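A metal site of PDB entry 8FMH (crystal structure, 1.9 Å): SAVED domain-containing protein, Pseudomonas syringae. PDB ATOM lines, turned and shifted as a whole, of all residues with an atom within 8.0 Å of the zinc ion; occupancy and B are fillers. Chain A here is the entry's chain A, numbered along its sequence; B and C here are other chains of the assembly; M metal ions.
Of the 20 residues printed, 4 come within 4 Å of the zinc ion. The nearest printed residue that does not touch the zinc ion is Leu 34 (4.6 Å).
The zinc ion is bound by the side-chain sulfur of Cys 90, the side-chain sulfur of Cys 87, the side-chain sulfur of Cys 35 and the side-chain sulfur of Cys 32. The zinc ion has four donor atoms within binding distance.
The side-chain hydroxyl of Thr 37 sits close to the side-chain sulfur of Cys 35, 3.0 Å away. N of Leu 34 sits close to SG of Cys 32 (3.5 Å). The backbone NH (N) of Cys 32 lies within hydrogen-bond range of the backbone carbonyl oxygen (O) of Thr 37 (2.9 Å).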
ATOM      1  N   HIS A  31      15.936  10.319 -11.683  1.00  0.00           N
ATOM      2  CA  HIS A  31      15.593  10.338 -10.273  1.00  0.00           C
ATOM      3  C   HIS A  31      16.397  11.401  -9.554  1.00  0.00           C
ATOM      4  O   HIS A  31      17.419  11.872 -10.052  1.00  0.00           O
ATOM      5  CB  HIS A  31      15.839   8.977  -9.608  1.00  0.00           C
ATOM      6  CG  HIS A  31      14.914   7.896 -10.080  1.00  0.00           C
ATOM      7  ND1 HIS A  31      14.058   7.226  -9.232  1.00  0.00           N
ATOM      8  CD2 HIS A  31      14.711   7.359 -11.304  1.00  0.00           C
ATOM      9  CE1 HIS A  31      13.368   6.335  -9.912  1.00  0.00           C
ATOM     10  NE2 HIS A  31      13.744   6.391 -11.171  1.00  0.00           N
ATOM     11  N   CYS A  32      15.919  11.782  -8.381  1.00  0.00           N
ATOM     12  CA  CYS A  32      16.626  12.750  -7.549  1.00  0.00           C
ATOM     13  C   CYS A  32      17.849  12.080  -6.928  1.00  0.00           C
ATOM     14  O   CYS A  32      17.738  11.045  -6.262  1.00  0.00           O
ATOM     15  CB  CYS A  32      15.704  13.291  -6.463  1.00  0.00           C
ATOM     16  SG  CYS A  32      16.474  14.489  -5.376  1.00  0.00           S
ATOM     17  N   GLU A  33      19.025  12.669  -7.152  1.00  0.00           N
ATOM     18  CA  GLU A  33      20.259  12.094  -6.634  1.00  0.00           C
ATOM     19  C   GLU A  33      20.340  12.144  -5.114  1.00  0.00           C
ATOM     20  O   GLU A  33      21.262  11.551  -4.543  1.00  0.00           O
ATOM     21  CB  GLU A  33      21.461  12.815  -7.225  1.00  0.00           C
ATOM     22  CG  GLU A  33      21.486  12.843  -8.733  1.00  0.00           C
ATOM     23  CD  GLU A  33      22.776  13.406  -9.280  1.00  0.00           C
ATOM     24  OE1 GLU A  33      23.800  13.315  -8.575  1.00  0.00           O
ATOM     25  OE2 GLU A  33      22.777  13.954 -10.410  1.00  0.00           O
ATOM     26  N   LEU A  34      19.408  12.817  -4.438  1.00  0.00           N
ATOM     27  CA  LEU A  34      19.482  12.987  -2.995  1.00  0.00           C
ATOM     28  C   LEU A  34      18.371  12.279  -2.229  1.00  0.00           C
ATOM     29  O   LEU A  34      18.589  11.952  -1.060  1.00  0.00           O
ATOM     30  CB  LEU A  34      19.451  14.484  -2.632  1.00  0.00           C
ATOM     31  CG  LEU A  34      20.718  15.289  -2.946  1.00  0.00           C
ATOM     32  CD1 LEU A  34      20.542  16.777  -2.657  1.00  0.00           C
ATOM     33  CD2 LEU A  34      21.900  14.749  -2.150  1.00  0.00           C
ATOM     34  N   CYS A  35      17.222  12.004  -2.843  1.00  0.00           N
ATOM     35  CA  CYS A  35      16.156  11.266  -2.162  1.00  0.00           C
ATOM     36  C   CYS A  35      15.584  10.120  -2.984  1.00  0.00           C
ATOM     37  O   CYS A  35      14.746   9.383  -2.478  1.00  0.00           O
ATOM     38  CB  CYS A  35      15.025  12.211  -1.748  1.00  0.00           C
ATOM     39  SG  CYS A  35      13.967  12.836  -3.082  1.00  0.00           S
ATOM     40  N   GLY A  36      16.005   9.954  -4.240  1.00  0.00           N
ATOM     41  CA  GLY A  36      15.604   8.802  -5.017  1.00  0.00           C
ATOM     42  C   GLY A  36      14.235   8.877  -5.640  1.00  0.00           C
ATOM     43  O   GLY A  36      13.824   7.917  -6.305  1.00  0.00           O
ATOM     44  N   THR A  37      13.491   9.973  -5.453  1.00  0.00           N
ATOM     45  CA  THR A  37      12.188  10.090  -6.073  1.00  0.00           C
ATOM     46  C   THR A  37      12.304  10.018  -7.593  1.00  0.00           C
ATOM     47  O   THR A  37      13.269  10.514  -8.168  1.00  0.00           O
ATOM     48  CB  THR A  37      11.504  11.394  -5.669  1.00  0.00           C
ATOM     49  OG1 THR A  37      11.541  11.552  -4.240  1.00  0.00           O
ATOM     50  CG2 THR A  37      10.056  11.405  -6.133  1.00  0.00           C
ATOM     51  N   ASP A  38      11.305   9.402  -8.220  1.00  0.00           N
ATOM     52  CA  ASP A  38      11.235   9.297  -9.669  1.00  0.00           C
ATOM     53  C   ASP A  38      10.639  10.587 -10.237  1.00  0.00           C
ATOM     54  O   ASP A  38       9.489  10.918  -9.968  1.00  0.00           O
ATOM     55  CB  ASP A  38      10.381   8.086 -10.053  1.00  0.00           C
ATOM     56  CG  ASP A  38      10.173   7.962 -11.557  1.00  0.00           C
ATOM     57  OD1 ASP A  38      10.746   8.774 -12.315  1.00  0.00           O
ATOM     58  OD2 ASP A  38       9.427   7.047 -11.962  1.00  0.00           O
ATOM     59  N   LEU A  39      11.437  11.305 -11.037  1.00  0.00           N
ATOM     60  CA  LEU A  39      11.074  12.634 -11.511  1.00  0.00           C
ATOM     61  C   LEU A  39      10.530  12.617 -12.934  1.00  0.00           C
ATOM     62  O   LEU A  39      10.412  13.691 -13.544  1.00  0.00           O
ATOM     63  CB  LEU A  39      12.287  13.560 -11.415  1.00  0.00           C
ATOM     64  CG  LEU A  39      12.843  13.731 -10.004  1.00  0.00           C
ATOM     65  CD1 LEU A  39      14.274  14.247 -10.047  1.00  0.00           C
ATOM     66  CD2 LEU A  39      11.972  14.666  -9.185  1.00  0.00           C
ATOM     67  N   TRP A  51       9.386  16.715 -13.669  1.00  0.00           N
ATOM     68  CA  TRP A  51       9.287  17.702 -12.599  1.00  0.00           C
ATOM     69  C   TRP A  51      10.576  17.794 -11.794  1.00  0.00           C
ATOM     70  O   TRP A  51      10.548  18.209 -10.634  1.00  0.00           O
ATOM     71  CB  TRP A  51       8.093  17.406 -11.700  1.00  0.00           C
ATOM     72  CG  TRP A  51       8.099  16.058 -11.020  1.00  0.00           C
ATOM     73  CD1 TRP A  51       7.939  14.833 -11.615  1.00  0.00           C
ATOM     74  CD2 TRP A  51       8.259  15.805  -9.620  1.00  0.00           C
ATOM     75  NE1 TRP A  51       7.997  13.837 -10.670  1.00  0.00           N
ATOM     76  CE2 TRP A  51       8.196  14.413  -9.434  1.00  0.00           C
ATOM     77  CE3 TRP A  51       8.467  16.622  -8.509  1.00  0.00           C
ATOM     78  CZ2 TRP A  51       8.331  13.819  -8.185  1.00  0.00           C
ATOM     79  CZ3 TRP A  51       8.595  16.040  -7.263  1.00  0.00           C
ATOM     80  CH2 TRP A  51       8.531  14.644  -7.110  1.00  0.00           C
ATOM     81  N   LEU A  85      20.748  16.237 -10.775  1.00  0.00           N
ATOM     82  CA  LEU A  85      19.306  16.211 -10.946  1.00  0.00           C
ATOM     83  C   LEU A  85      18.686  16.058  -9.568  1.00  0.00           C
ATOM     84  O   LEU A  85      18.911  15.055  -8.881  1.00  0.00           O
ATOM     85  CB  LEU A  85      18.859  15.072 -11.869  1.00  0.00           C
ATOM     86  CG  LEU A  85      17.358  15.071 -12.176  1.00  0.00           C
ATOM     87  CD1 LEU A  85      17.001  16.272 -13.039  1.00  0.00           C
ATOM     88  CD2 LEU A  85      16.900  13.786 -12.847  1.00  0.00           C
ATOM     89  N   LEU A  86      17.913  17.058  -9.166  1.00  0.00           N
ATOM     90  CA  LEU A  86      17.297  17.082  -7.850  1.00  0.00           C
ATOM     91  C   LEU A  86      15.794  17.258  -8.003  1.00  0.00           C
ATOM     92  O   LEU A  86      15.300  17.779  -9.014  1.00  0.00           O
ATOM     93  CB  LEU A  86      17.883  18.201  -6.984  1.00  0.00           C
ATOM     94  CG  LEU A  86      19.366  18.056  -6.642  1.00  0.00           C
ATOM     95  CD1 LEU A  86      19.834  19.214  -5.770  1.00  0.00           C
ATOM     96  CD2 LEU A  86      19.657  16.719  -5.965  1.00  0.00           C
ATOM     97  N   CYS A  87      15.045  16.804  -7.000  1.00  0.00           N
ATOM     98  CA  CYS A  87      13.638  17.120  -6.974  1.00  0.00           C
ATOM     99  C   CYS A  87      13.485  18.577  -6.530  1.00  0.00           C
ATOM    100  O   CYS A  87      14.388  19.159  -5.928  1.00  0.00           O
ATOM    101  CB  CYS A  87      12.889  16.166  -6.041  1.00  0.00           C
ATOM    102  SG  CYS A  87      13.217  16.372  -4.304  1.00  0.00           S
ATOM    103  N   PRO A  88      12.346  19.201  -6.849  1.00  0.00           N
ATOM    104  CA  PRO A  88      12.187  20.617  -6.504  1.00  0.00           C
ATOM    105  C   PRO A  88      12.451  20.932  -5.032  1.00  0.00           C
ATOM    106  O   PRO A  88      12.987  22.000  -4.722  1.00  0.00           O
ATOM    107  CB  PRO A  88      10.734  20.888  -6.901  1.00  0.00           C
ATOM    108  CG  PRO A  88      10.510  19.965  -8.036  1.00  0.00           C
ATOM    109  CD  PRO A  88      11.229  18.701  -7.664  1.00  0.00           C
ATOM    110  N   GLY A  89      12.116  20.017  -4.123  1.00  0.00           N
ATOM    111  CA  GLY A  89      12.324  20.265  -2.708  1.00  0.00           C
ATOM    112  C   GLY A  89      13.765  20.091  -2.255  1.00  0.00           C
ATOM    113  O   GLY A  89      14.258  20.859  -1.424  1.00  0.00           O
ATOM    114  N   CYS A  90      14.447  19.063  -2.777  1.00  0.00           N
ATOM    115  CA  CYS A  90      15.855  18.880  -2.449  1.00  0.00           C
ATOM    116  C   CYS A  90      16.709  20.014  -3.005  1.00  0.00           C
ATOM    117  O   CYS A  90      17.803  20.272  -2.497  1.00  0.00           O
ATOM    118  CB  CYS A  90      16.355  17.533  -2.978  1.00  0.00           C
ATOM    119  SG  CYS A  90      15.760  16.110  -2.032  1.00  0.00           S
ATOM    120  N   HIS A  91      16.218  20.692  -4.040  1.00  0.00           N
ATOM    121  CA  HIS A  91      16.909  21.831  -4.614  1.00  0.00           C
ATOM    122  C   HIS A  91      16.759  23.070  -3.733  1.00  0.00           C
ATOM    123  O   HIS A  91      17.747  23.781  -3.482  1.00  0.00           O
ATOM    124  CB  HIS A  91      16.366  22.088  -6.015  1.00  0.00           C
ATOM    125  CG  HIS A  91      17.269  22.904  -6.881  1.00  0.00           C
ATOM    126  ND1 HIS A  91      16.978  23.166  -8.206  1.00  0.00           N
ATOM    127  CD2 HIS A  91      18.455  23.521  -6.631  1.00  0.00           C
ATOM    128  CE1 HIS A  91      17.936  23.912  -8.726  1.00  0.00           C
ATOM    129  NE2 HIS A  91      18.843  24.135  -7.789  1.00  0.00           N
ATOM    130  N   LYS A  93      16.356  23.069  -0.622  1.00  0.00           N
ATOM    131  CA  LYS A  93      17.039  22.855   0.643  1.00  0.00           C
ATOM    132  C   LYS A  93      18.550  23.059   0.527  1.00  0.00           C
ATOM    133  O   LYS A  93      19.162  23.714   1.376  1.00  0.00           O
ATOM    134  CB  LYS A  93      16.725  21.457   1.169  1.00  0.00           C
ATOM    135  CG  LYS A  93      15.319  21.321   1.721  1.00  0.00           C
ATOM    136  CD  LYS A  93      14.870  19.863   1.747  1.00  0.00           C
ATOM    137  CE  LYS A  93      13.539  19.714   2.461  1.00  0.00           C
ATOM    138  NZ  LYS A  93      13.014  18.328   2.357  1.00  0.00           N
ATOM    139  N   ARG B  44      16.832  16.840   7.151  1.00  0.00           N
ATOM    140  CA  ARG B  44      18.064  16.155   6.780  1.00  0.00           C
ATOM    141  C   ARG B  44      19.296  16.854   7.360  1.00  0.00           C
ATOM    142  O   ARG B  44      20.184  16.203   7.912  1.00  0.00           O
ATOM    143  CB  ARG B  44      18.184  16.053   5.258  1.00  0.00           C
ATOM    144  CG  ARG B  44      19.547  15.532   4.804  1.00  0.00           C
ATOM    145  CD  ARG B  44      19.579  15.187   3.329  1.00  0.00           C
ATOM    146  NE  ARG B  44      20.882  14.698   2.919  1.00  0.00           N
ATOM    147  CZ  ARG B  44      21.107  13.954   1.848  1.00  0.00           C
ATOM    148  NH1 ARG B  44      20.122  13.590   1.036  1.00  0.00           N
ATOM    149  NH2 ARG B  44      22.343  13.545   1.575  1.00  0.00           N
ATOM    150  N   PRO C 124      19.155   6.310  -2.952  1.00  0.00           N
ATOM    151  CA  PRO C 124      19.139   7.391  -1.953  1.00  0.00           C
ATOM    152  C   PRO C 124      18.074   7.222  -0.874  1.00  0.00           C
ATOM    153  O   PRO C 124      18.301   7.641   0.273  1.00  0.00           O
ATOM    154  CB  PRO C 124      18.915   8.653  -2.791  1.00  0.00           C
ATOM    155  CG  PRO C 124      19.519   8.313  -4.116  1.00  0.00           C
ATOM    156  CD  PRO C 124      19.239   6.851  -4.330  1.00  0.00           C
HETATM  157 ZN    ZN M   1      14.874  14.861  -3.737  1.00  0.00          ZN
